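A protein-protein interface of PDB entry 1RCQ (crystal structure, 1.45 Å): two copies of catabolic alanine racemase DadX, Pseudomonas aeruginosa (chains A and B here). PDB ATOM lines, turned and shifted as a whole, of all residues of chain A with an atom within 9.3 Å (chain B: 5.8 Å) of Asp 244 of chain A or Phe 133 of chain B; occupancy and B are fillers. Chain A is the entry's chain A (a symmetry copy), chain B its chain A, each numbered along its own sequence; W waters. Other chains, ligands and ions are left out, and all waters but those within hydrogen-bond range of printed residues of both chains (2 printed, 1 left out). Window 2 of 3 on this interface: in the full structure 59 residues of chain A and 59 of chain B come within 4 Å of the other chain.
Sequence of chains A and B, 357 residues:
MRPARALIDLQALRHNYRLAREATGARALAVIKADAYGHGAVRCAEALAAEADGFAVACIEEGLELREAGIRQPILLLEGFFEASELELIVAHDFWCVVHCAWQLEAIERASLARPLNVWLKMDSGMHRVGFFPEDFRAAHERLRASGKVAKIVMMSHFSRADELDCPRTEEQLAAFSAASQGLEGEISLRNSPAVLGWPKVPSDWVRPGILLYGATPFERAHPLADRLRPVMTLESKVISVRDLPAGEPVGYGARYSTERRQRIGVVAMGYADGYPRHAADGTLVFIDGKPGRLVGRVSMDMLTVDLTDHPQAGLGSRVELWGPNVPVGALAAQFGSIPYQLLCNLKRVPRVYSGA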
ATOM      1  N   SER A 241     -16.705   9.457   7.037  1.00  0.00           N
ATOM      2  CA  SER A 241     -16.355   9.525   5.634  1.00  0.00           C
ATOM      3  C   SER A 241     -14.866   9.244   5.469  1.00  0.00           C
ATOM      4  O   SER A 241     -14.054   9.571   6.335  1.00  0.00           O
ATOM      5  CB  SER A 241     -16.700  10.891   4.966  1.00  0.00           C
ATOM      6  OG  SER A 241     -16.140  10.882   3.654  1.00  0.00           O
ATOM      7  N   VAL A 242     -14.449   8.611   4.366  1.00  0.00           N
ATOM      8  CA  VAL A 242     -13.057   8.321   4.048  1.00  0.00           C
ATOM      9  C   VAL A 242     -12.773   8.874   2.653  1.00  0.00           C
ATOM     10  O   VAL A 242     -13.646   8.868   1.781  1.00  0.00           O
ATOM     11  CB  VAL A 242     -12.783   6.805   4.103  1.00  0.00           C
ATOM     12  CG1 VAL A 242     -11.417   6.396   3.599  1.00  0.00           C
ATOM     13  CG2 VAL A 242     -12.942   6.309   5.555  1.00  0.00           C
ATOM     14  N   ARG A 243     -11.564   9.366   2.476  1.00  0.00           N
ATOM     15  CA  ARG A 243     -11.141   9.957   1.223  1.00  0.00           C
ATOM     16  C   ARG A 243      -9.706   9.615   0.886  1.00  0.00           C
ATOM     17  O   ARG A 243      -8.847   9.817   1.750  1.00  0.00           O
ATOM     18  CB  ARG A 243     -11.243  11.492   1.366  1.00  0.00           C
ATOM     19  CG  ARG A 243     -10.909  12.362   0.235  1.00  0.00           C
ATOM     20  CD  ARG A 243     -11.345  13.817   0.362  1.00  0.00           C
ATOM     21  NE  ARG A 243     -12.698  13.880   0.887  1.00  0.00           N
ATOM     22  CZ  ARG A 243     -13.786  13.772   0.163  1.00  0.00           C
ATOM     23  NH1 ARG A 243     -13.754  13.631  -1.156  1.00  0.00           N
ATOM     24  NH2 ARG A 243     -14.920  13.829   0.827  1.00  0.00           N
ATOM     25  N   ASP A 244      -9.403   9.125  -0.294  1.00  0.00           N
ATOM     26  CA  ASP A 244      -8.042   8.982  -0.765  1.00  0.00           C
ATOM     27  C   ASP A 244      -7.590  10.260  -1.508  1.00  0.00           C
ATOM     28  O   ASP A 244      -8.325  10.748  -2.384  1.00  0.00           O
ATOM     29  CB  ASP A 244      -7.863   7.815  -1.713  1.00  0.00           C
ATOM     30  CG  ASP A 244      -8.189   6.423  -1.220  1.00  0.00           C
ATOM     31  OD1 ASP A 244      -7.937   6.083  -0.060  1.00  0.00           O
ATOM     32  OD2 ASP A 244      -8.711   5.627  -2.020  1.00  0.00           O
ATOM     33  N   LEU A 245      -6.423  10.770  -1.158  1.00  0.00           N
ATOM     34  CA  LEU A 245      -5.876  12.001  -1.701  1.00  0.00           C
ATOM     35  C   LEU A 245      -4.466  11.815  -2.217  1.00  0.00           C
ATOM     36  O   LEU A 245      -3.690  11.136  -1.552  1.00  0.00           O
ATOM     37  CB  LEU A 245      -5.789  13.088  -0.630  1.00  0.00           C
ATOM     38  CG  LEU A 245      -7.152  13.668  -0.204  1.00  0.00           C
ATOM     39  CD1 LEU A 245      -6.955  14.629   0.957  1.00  0.00           C
ATOM     40  CD2 LEU A 245      -7.869  14.346  -1.368  1.00  0.00           C
ATOM     41  N   PRO A 246      -4.138  12.424  -3.343  1.00  0.00           N
ATOM     42  CA  PRO A 246      -2.736  12.506  -3.732  1.00  0.00           C
ATOM     43  C   PRO A 246      -2.014  13.422  -2.747  1.00  0.00           C
ATOM     44  O   PRO A 246      -2.605  14.091  -1.911  1.00  0.00           O
ATOM     45  CB  PRO A 246      -2.806  13.123  -5.120  1.00  0.00           C
ATOM     46  CG  PRO A 246      -4.169  13.632  -5.360  1.00  0.00           C
ATOM     47  CD  PRO A 246      -5.047  13.082  -4.293  1.00  0.00           C
ATOM     48  N   ALA A 247      -0.697  13.464  -2.851  1.00  0.00           N
ATOM     49  CA  ALA A 247       0.143  14.355  -2.091  1.00  0.00           C
ATOM     50  C   ALA A 247      -0.075  15.810  -2.521  1.00  0.00           C
ATOM     51  O   ALA A 247      -0.336  16.123  -3.680  1.00  0.00           O
ATOM     52  CB  ALA A 247       1.591  13.964  -2.354  1.00  0.00           C
ATOM     53  N   GLU A 249      -2.316  18.000  -1.183  1.00  0.00           N
ATOM     54  CA  GLU A 249      -3.696  18.440  -1.198  1.00  0.00           C
ATOM     55  C   GLU A 249      -4.057  19.008   0.184  1.00  0.00           C
ATOM     56  O   GLU A 249      -3.777  18.384   1.197  1.00  0.00           O
ATOM     57  CB  GLU A 249      -4.651  17.312  -1.550  1.00  0.00           C
ATOM     58  CG  GLU A 249      -4.521  16.888  -3.011  1.00  0.00           C
ATOM     59  CD  GLU A 249      -5.075  17.951  -3.940  1.00  0.00           C
ATOM     60  OE1 GLU A 249      -6.064  18.651  -3.604  1.00  0.00           O
ATOM     61  OE2 GLU A 249      -4.492  18.100  -5.048  1.00  0.00           O
ATOM     62  N   PRO A 250      -4.650  20.186   0.183  1.00  0.00           N
ATOM     63  CA  PRO A 250      -4.980  20.875   1.427  1.00  0.00           C
ATOM     64  C   PRO A 250      -6.182  20.222   2.101  1.00  0.00           C
ATOM     65  O   PRO A 250      -7.138  19.845   1.405  1.00  0.00           O
ATOM     66  CB  PRO A 250      -5.318  22.308   0.972  1.00  0.00           C
ATOM     67  CG  PRO A 250      -5.841  22.126  -0.413  1.00  0.00           C
ATOM     68  CD  PRO A 250      -5.060  20.976  -0.995  1.00  0.00           C
ATOM     69  N   VAL A 251      -6.108  20.075   3.410  1.00  0.00           N
ATOM     70  CA  VAL A 251      -7.219  19.470   4.140  1.00  0.00           C
ATOM     71  C   VAL A 251      -7.809  20.468   5.140  1.00  0.00           C
ATOM     72  O   VAL A 251      -7.121  20.926   6.049  1.00  0.00           O
ATOM     73  CB  VAL A 251      -6.793  18.209   4.886  1.00  0.00           C
ATOM     74  CG1 VAL A 251      -8.005  17.538   5.544  1.00  0.00           C
ATOM     75  CG2 VAL A 251      -6.091  17.235   3.944  1.00  0.00           C
ATOM     76  N   THR A 259      -1.589  17.222   2.399  1.00  0.00           N
ATOM     77  CA  THR A 259      -1.076  15.844   2.471  1.00  0.00           C
ATOM     78  C   THR A 259       0.409  15.800   2.111  1.00  0.00           C
ATOM     79  O   THR A 259       0.817  16.426   1.120  1.00  0.00           O
ATOM     80  CB  THR A 259      -1.871  14.897   1.580  1.00  0.00           C
ATOM     81  OG1 THR A 259      -1.942  15.463   0.277  1.00  0.00           O
ATOM     82  CG2 THR A 259      -3.298  14.767   2.139  1.00  0.00           C
ATOM     83  N   ARG A 261       2.101  12.924   1.461  1.00  0.00           N
ATOM     84  CA  ARG A 261       2.152  11.859   0.492  1.00  0.00           C
ATOM     85  C   ARG A 261       0.745  11.455   0.072  1.00  0.00           C
ATOM     86  O   ARG A 261      -0.222  12.092   0.497  1.00  0.00           O
ATOM     87  CB  ARG A 261       2.762  10.615   1.153  1.00  0.00           C
ATOM     88  CG  ARG A 261       4.144  10.849   1.731  1.00  0.00           C
ATOM     89  CD  ARG A 261       4.772   9.543   2.117  1.00  0.00           C
ATOM     90  NE  ARG A 261       6.161   9.712   2.522  1.00  0.00           N
ATOM     91  CZ  ARG A 261       7.235   9.587   1.747  1.00  0.00           C
ATOM     92  NH1 ARG A 261       7.128   9.302   0.448  1.00  0.00           N
ATOM     93  NH2 ARG A 261       8.415   9.779   2.331  1.00  0.00           N
ATOM     94  N   ARG A 262       0.669  10.385  -0.715  1.00  0.00           N
ATOM     95  CA  ARG A 262      -0.645   9.831  -1.036  1.00  0.00           C
ATOM     96  C   ARG A 262      -1.199   9.344   0.303  1.00  0.00           C
ATOM     97  O   ARG A 262      -0.538   8.576   1.015  1.00  0.00           O
ATOM     98  CB  ARG A 262      -0.492   8.682  -2.033  1.00  0.00           C
ATOM     99  CG  ARG A 262      -0.237   9.125  -3.454  1.00  0.00           C
ATOM    100  CD  ARG A 262       0.080   8.003  -4.413  1.00  0.00           C
ATOM    101  NE  ARG A 262       1.284   7.315  -3.949  1.00  0.00           N
ATOM    102  CZ  ARG A 262       1.612   6.071  -4.244  1.00  0.00           C
ATOM    103  NH1 ARG A 262       0.838   5.336  -5.035  1.00  0.00           N
ATOM    104  NH2 ARG A 262       2.719   5.517  -3.771  1.00  0.00           N
ATOM    105  N   GLN A 263      -2.386   9.777   0.676  1.00  0.00           N
ATOM    106  CA  GLN A 263      -2.929   9.470   1.993  1.00  0.00           C
ATOM    107  C   GLN A 263      -4.397   9.176   1.881  1.00  0.00           C
ATOM    108  O   GLN A 263      -5.059   9.516   0.927  1.00  0.00           O
ATOM    109  CB  GLN A 263      -2.740  10.681   2.908  1.00  0.00           C
ATOM    110  CG  GLN A 263      -1.281  10.807   3.311  1.00  0.00           C
ATOM    111  CD  GLN A 263      -1.136  11.959   4.282  1.00  0.00           C
ATOM    112  OE1 GLN A 263      -0.374  12.855   4.008  1.00  0.00           O
ATOM    113  NE2 GLN A 263      -1.868  11.871   5.376  1.00  0.00           N
ATOM    114  N   ARG A 264      -4.934   8.536   2.876  1.00  0.00           N
ATOM    115  CA  ARG A 264      -6.286   8.245   3.220  1.00  0.00           C
ATOM    116  C   ARG A 264      -6.649   9.021   4.489  1.00  0.00           C
ATOM    117  O   ARG A 264      -6.025   8.823   5.532  1.00  0.00           O
ATOM    118  CB  ARG A 264      -6.520   6.742   3.443  1.00  0.00           C
ATOM    119  CG  ARG A 264      -8.010   6.388   3.325  1.00  0.00           C
ATOM    120  CD  ARG A 264      -8.207   4.888   3.112  1.00  0.00           C
ATOM    121  NE  ARG A 264      -7.654   4.154   4.242  1.00  0.00           N
ATOM    122  CZ  ARG A 264      -8.278   3.412   5.148  1.00  0.00           C
ATOM    123  NH1 ARG A 264      -9.597   3.215   5.142  1.00  0.00           N
ATOM    124  NH2 ARG A 264      -7.517   2.848   6.092  1.00  0.00           N
ATOM    125  N   ILE A 265      -7.628   9.895   4.328  1.00  0.00           N
ATOM    126  CA  ILE A 265      -8.098  10.738   5.425  1.00  0.00           C
ATOM    127  C   ILE A 265      -9.497  10.307   5.835  1.00  0.00           C
ATOM    128  O   ILE A 265     -10.332   9.902   5.018  1.00  0.00           O
ATOM    129  CB  ILE A 265      -8.013  12.217   5.000  1.00  0.00           C
ATOM    130  CG1 ILE A 265      -6.576  12.586   4.592  1.00  0.00           C
ATOM    131  CG2 ILE A 265      -8.575  13.164   6.043  1.00  0.00           C
ATOM    132  CD1 ILE A 265      -5.506  12.136   5.552  1.00  0.00           C
ATOM    133  N   GLY A 266      -9.745  10.351   7.147  1.00  0.00           N
ATOM    134  CA  GLY A 266     -11.062  10.050   7.682  1.00  0.00           C
ATOM    135  C   GLY A 266     -11.636  11.283   8.357  1.00  0.00           C
ATOM    136  O   GLY A 266     -10.922  11.973   9.078  1.00  0.00           O
ATOM    137  N   LEU A 308      -5.645   8.138   8.202  1.00  0.00           N
ATOM    138  CA  LEU A 308      -5.903   6.699   8.218  1.00  0.00           C
ATOM    139  C   LEU A 308      -4.897   5.939   7.370  1.00  0.00           C
ATOM    140  O   LEU A 308      -5.056   4.741   7.138  1.00  0.00           O
ATOM    141  CB  LEU A 308      -7.317   6.429   7.702  1.00  0.00           C
ATOM    142  CG  LEU A 308      -8.517   6.902   8.517  1.00  0.00           C
ATOM    143  CD1 LEU A 308      -9.851   6.607   7.859  1.00  0.00           C
ATOM    144  CD2 LEU A 308      -8.447   6.275   9.905  1.00  0.00           C
ATOM    145  N   THR A 309      -3.847   6.602   6.875  1.00  0.00           N
ATOM    146  CA  THR A 309      -2.973   5.951   5.894  1.00  0.00           C
ATOM    147  C   THR A 309      -2.302   4.686   6.421  1.00  0.00           C
ATOM    148  O   THR A 309      -2.264   3.716   5.656  1.00  0.00           O
ATOM    149  CB  THR A 309      -1.881   6.932   5.458  1.00  0.00           C
ATOM    150  OG1 THR A 309      -2.532   8.167   5.105  1.00  0.00           O
ATOM    151  CG2 THR A 309      -1.091   6.400   4.274  1.00  0.00           C
ATOM    152  N   ALA A 314      -8.706   0.221   9.337  1.00  0.00           N
ATOM    153  CA  ALA A 314      -9.666   1.208   9.816  1.00  0.00           C
ATOM    154  C   ALA A 314     -10.397   1.860   8.652  1.00  0.00           C
ATOM    155  O   ALA A 314      -9.905   1.849   7.520  1.00  0.00           O
ATOM    156  CB  ALA A 314      -8.956   2.262  10.661  1.00  0.00           C
ATOM    157  N   MET B 123     -20.419  18.184  -3.352  1.00  0.00           N
ATOM    158  CA  MET B 123     -19.141  17.961  -3.965  1.00  0.00           C
ATOM    159  C   MET B 123     -17.978  18.444  -3.111  1.00  0.00           C
ATOM    160  O   MET B 123     -18.038  19.511  -2.490  1.00  0.00           O
ATOM    161  CB  MET B 123     -19.081  18.747  -5.302  1.00  0.00           C
ATOM    162  CG  MET B 123     -17.926  18.384  -6.202  1.00  0.00           C
ATOM    163  SD  MET B 123     -17.653  19.436  -7.643  1.00  0.00           S
ATOM    164  CE  MET B 123     -19.207  19.359  -8.518  1.00  0.00           C
ATOM    165  N   ASP B 124     -16.914  17.664  -3.113  1.00  0.00           N
ATOM    166  CA  ASP B 124     -15.663  18.093  -2.500  1.00  0.00           C
ATOM    167  C   ASP B 124     -14.971  18.847  -3.650  1.00  0.00           C
ATOM    168  O   ASP B 124     -14.418  18.198  -4.547  1.00  0.00           O
ATOM    169  CB  ASP B 124     -14.818  16.942  -1.996  1.00  0.00           C
ATOM    170  CG  ASP B 124     -13.389  17.335  -1.678  1.00  0.00           C
ATOM    171  OD1 ASP B 124     -13.083  18.558  -1.617  1.00  0.00           O
ATOM    172  OD2 ASP B 124     -12.566  16.415  -1.509  1.00  0.00           O
ATOM    173  N   HIS B 128     -11.667  19.155   0.792  1.00  0.00           N
ATOM    174  CA  HIS B 128     -11.325  17.811   1.243  1.00  0.00           C
ATOM    175  C   HIS B 128     -11.799  17.537   2.671  1.00  0.00           C
ATOM    176  O   HIS B 128     -11.083  16.936   3.501  1.00  0.00           O
ATOM    177  CB  HIS B 128      -9.815  17.594   1.086  1.00  0.00           C
ATOM    178  CG  HIS B 128      -9.359  17.759  -0.335  1.00  0.00           C
ATOM    179  ND1 HIS B 128     -10.067  17.331  -1.428  1.00  0.00           N
ATOM    180  CD2 HIS B 128      -8.252  18.349  -0.833  1.00  0.00           C
ATOM    181  CE1 HIS B 128      -9.415  17.632  -2.540  1.00  0.00           C
ATOM    182  NE2 HIS B 128      -8.286  18.260  -2.211  1.00  0.00           N
ATOM    183  N   GLY B 131     -17.943  15.153   0.807  1.00  0.00           N
ATOM    184  CA  GLY B 131     -18.464  15.234  -0.523  1.00  0.00           C
ATOM    185  C   GLY B 131     -17.807  14.352  -1.559  1.00  0.00           C
ATOM    186  O   GLY B 131     -16.745  13.777  -1.368  1.00  0.00           O
ATOM    187  N   PHE B 132     -18.466  14.221  -2.707  1.00  0.00           N
ATOM    188  CA  PHE B 132     -17.917  13.447  -3.806  1.00  0.00           C
ATOM    189  C   PHE B 132     -16.867  14.249  -4.548  1.00  0.00           C
ATOM    190  O   PHE B 132     -17.008  15.453  -4.748  1.00  0.00           O
ATOM    191  CB  PHE B 132     -19.045  13.075  -4.795  1.00  0.00           C
ATOM    192  CG  PHE B 132     -20.071  12.115  -4.221  1.00  0.00           C
ATOM    193  CD1 PHE B 132     -21.190  12.596  -3.572  1.00  0.00           C
ATOM    194  CD2 PHE B 132     -19.885  10.737  -4.301  1.00  0.00           C
ATOM    195  CE1 PHE B 132     -22.109  11.726  -3.027  1.00  0.00           C
ATOM    196  CE2 PHE B 132     -20.822   9.872  -3.776  1.00  0.00           C
ATOM    197  CZ  PHE B 132     -21.928  10.352  -3.128  1.00  0.00           C
ATOM    198  N   PHE B 133     -15.808  13.570  -4.970  1.00  0.00           N
ATOM    199  CA  PHE B 133     -14.854  14.216  -5.873  1.00  0.00           C
ATOM    200  C   PHE B 133     -15.527  14.663  -7.155  1.00  0.00           C
ATOM    201  O   PHE B 133     -16.516  14.041  -7.557  1.00  0.00           O
ATOM    202  CB  PHE B 133     -13.746  13.224  -6.169  1.00  0.00           C
ATOM    203  CG  PHE B 133     -12.694  13.078  -5.084  1.00  0.00           C
ATOM    204  CD1 PHE B 133     -12.111  14.193  -4.496  1.00  0.00           C
ATOM    205  CD2 PHE B 133     -12.291  11.824  -4.685  1.00  0.00           C
ATOM    206  CE1 PHE B 133     -11.131  14.046  -3.535  1.00  0.00           C
ATOM    207  CE2 PHE B 133     -11.313  11.681  -3.714  1.00  0.00           C
ATOM    208  CZ  PHE B 133     -10.729  12.776  -3.138  1.00  0.00           C
ATOM    209  N   PRO B 134     -15.019  15.711  -7.780  1.00  0.00           N
ATOM    210  CA  PRO B 134     -15.639  16.183  -9.026  1.00  0.00           C
ATOM    211  C   PRO B 134     -15.869  15.087 -10.057  1.00  0.00           C
ATOM    212  O   PRO B 134     -16.918  14.990 -10.713  1.00  0.00           O
ATOM    213  CB  PRO B 134     -14.606  17.209  -9.529  1.00  0.00           C
ATOM    214  CG  PRO B 134     -14.031  17.744  -8.259  1.00  0.00           C
ATOM    215  CD  PRO B 134     -13.867  16.526  -7.386  1.00  0.00           C
ATOM    216  N   GLU B 135     -14.888  14.204 -10.208  1.00  0.00           N
ATOM    217  CA  GLU B 135     -14.983  13.128 -11.183  1.00  0.00           C
ATOM    218  C   GLU B 135     -16.041  12.088 -10.825  1.00  0.00           C
ATOM    219  O   GLU B 135     -16.425  11.315 -11.716  1.00  0.00           O
ATOM    220  CB  GLU B 135     -13.612  12.444 -11.324  1.00  0.00           C
ATOM    221  CG  GLU B 135     -13.045  12.006  -9.982  1.00  0.00           C
ATOM    222  CD  GLU B 135     -12.001  12.907  -9.342  1.00  0.00           C
ATOM    223  OE1 GLU B 135     -12.114  14.158  -9.416  1.00  0.00           O
ATOM    224  OE2 GLU B 135     -11.065  12.325  -8.729  1.00  0.00           O
ATOM    225  N   ASP B 136     -16.533  12.047  -9.605  1.00  0.00           N
ATOM    226  CA  ASP B 136     -17.554  11.102  -9.166  1.00  0.00           C
ATOM    227  C   ASP B 136     -18.940  11.727  -9.058  1.00  0.00           C
ATOM    228  O   ASP B 136     -19.925  11.025  -8.805  1.00  0.00           O
ATOM    229  CB  ASP B 136     -17.172  10.500  -7.803  1.00  0.00           C
ATOM    230  CG  ASP B 136     -15.861   9.747  -7.812  1.00  0.00           C
ATOM    231  OD1 ASP B 136     -15.630   8.978  -8.773  1.00  0.00           O
ATOM    232  OD2 ASP B 136     -15.027   9.857  -6.901  1.00  0.00           O
ATOM    233  N   PHE B 137     -19.032  13.025  -9.262  1.00  0.00           N
ATOM    234  CA  PHE B 137     -20.239  13.773  -8.942  1.00  0.00           C
ATOM    235  C   PHE B 137     -21.369  13.479  -9.899  1.00  0.00           C
ATOM    236  O   PHE B 137     -22.498  13.310  -9.448  1.00  0.00           O
ATOM    237  CB  PHE B 137     -19.941  15.275  -8.936  1.00  0.00           C
ATOM    238  CG  PHE B 137     -21.024  16.201  -8.421  1.00  0.00           C
ATOM    239  CD1 PHE B 137     -21.232  16.424  -7.070  1.00  0.00           C
ATOM    240  CD2 PHE B 137     -21.859  16.874  -9.295  1.00  0.00           C
ATOM    241  CE1 PHE B 137     -22.225  17.291  -6.624  1.00  0.00           C
ATOM    242  CE2 PHE B 137     -22.840  17.735  -8.856  1.00  0.00           C
ATOM    243  CZ  PHE B 137     -23.040  17.959  -7.508  1.00  0.00           C
HETATM  244  O   HOH W   1     -11.678  14.385   3.881  1.00  0.00           O
HETATM  245  O   HOH W   2     -17.718  12.523   2.269  1.00  0.00           O
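Water W1 bridges the backbone carbonyl oxygen (O) of His 128 of chain B (2.6 Å) and the guanidinium group (NE) of Arg 243 of chain A (3.2 Å). Water W2 lies within hydrogen-bond range of OG of Ser 241 of chain A (2.7 Å), N of Gly 131 of chain B (3.0 Å) and NH2 of Arg 243 of chain A (3.4 Å).
Phe 133 of chain B touches Arg 243 of chain A (CZ to CG, 3.4 Å). O of Asp 244 of chain A touches CZ of Phe 133 of chain B, at 3.2 Å. His 128 of chain B touches Leu 245 of chain A. CD2 of Leu 245 of chain A touches CZ of Phe 133 of chain B, 3.7 Å away. His 128 of chain B touches Pro 250 of chain A. CG1 of Val 251 of chain A touches O of His 128 of chain B, at 3.7 Å.
No position is printed for both chains. Of the 9 pairs that touch across the chains among the printed residues, none has its exchanged pair printed and touching as well.
Hydrophobic or aromatic side chains of chain A that line the printed part of chain B: Leu 245 and Val 251. Of the 10 printed residues of chain B, 4 touch a printed residue of chain A. Hydrophobic or aromatic side chains of chain B that line the printed part of chain A: His 128 and Phe 133. Among the printed residues, 9 pairs touch across the chains. Among the printed residues, Asp or Glu carboxylates within 4 Å of a Lys or Arg side-chain nitrogen of the other chain: Arg 243 of chain A with Asp 124 of chain B (3.0 Å).
Of chain B, only Phe 133 (3.2 Å) comes within 4 Å of Asp 244 of chain A. Phe 133 of chain B touches just these residues of chain A: Arg 243 (3.4 Å), Asp 244 (3.2 Å) and Leu 245 (3.7 Å). No residue of chain A comes within 4 Å of Pro 134 of chain B. No residue of chain A comes within 4 Å of Glu 135 of chain B. Printed residues of chain B within 4 Å of Val 251 of chain A: His 128. Of the printed residues of chain A, His 128 of chain B touches Leu 245 (3.7 Å), Glu 249 (2.7 Å), Pro 250 (2.9 Å) and Val 251 (3.7 Å). Printed residues of chain A within 4 Å of Gly 131 of chain B: Arg 243 (2.9 Å). Of the printed residues of chain B, Arg 243 of chain A touches Asp 124 (3.0 Å), Gly 131 (2.9 Å) and Phe 133 (3.4 Å). Of the printed residues of chain B, Glu 249 of chain A touches His 128 (2.7 Å). Gly 266 of chain A touches none of the printed residues of chain B. The nearest printed residue of chain B that does not touch Asp 244 of chain A is His 128 of chain B (6.9 Å). The nearest residue of chain A that does not touch Phe 133 of chain B is Pro 246 of chain A (5.8 Å). The nearest printed residue of chain B that does not touch Leu 245 of chain A is Asp 124 of chain B (5.1 Å).
The guanidinium group (NH1) of Arg 243 of chain A lies within salt-bridge range of the side-chain carboxylate (OD2) of Asp 124 of chain B, 3.0 Å away. A ring nitrogen (NE2) of His 128 of chain B is in hydrogen-bond range of the side-chain carboxylate (OE1) of Glu 249 of chain A (2.7 Å). O of Gly 131 of chain B sits at hydrogen-bond distance from NH2 of Arg 243 of chain A (2.9 Å).
ND1 of His 128 of chain B is in hydrogen-bond range of OD2 of Asp 124 of chain B (2.7 Å). The backbone carbonyl oxygen of Phe 132 of chain B is in hydrogen-bond range of the backbone NH of Asp 124 of chain B (2.8 Å). N of Ile 265 of chain A is in hydrogen-bond range of O of Arg 243 of chain A, at 2.9 Å. The backbone NH (N) of Leu 245 of chain A sits at hydrogen-bond distance from the backbone carbonyl oxygen (O) of Gln 263 of chain A, at 2.8 Å. The backbone carbonyl oxygen (O) of Glu 249 of chain A lies within hydrogen-bond range of the backbone NH (N) of Thr 259 of chain A, 2.8 Å away.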
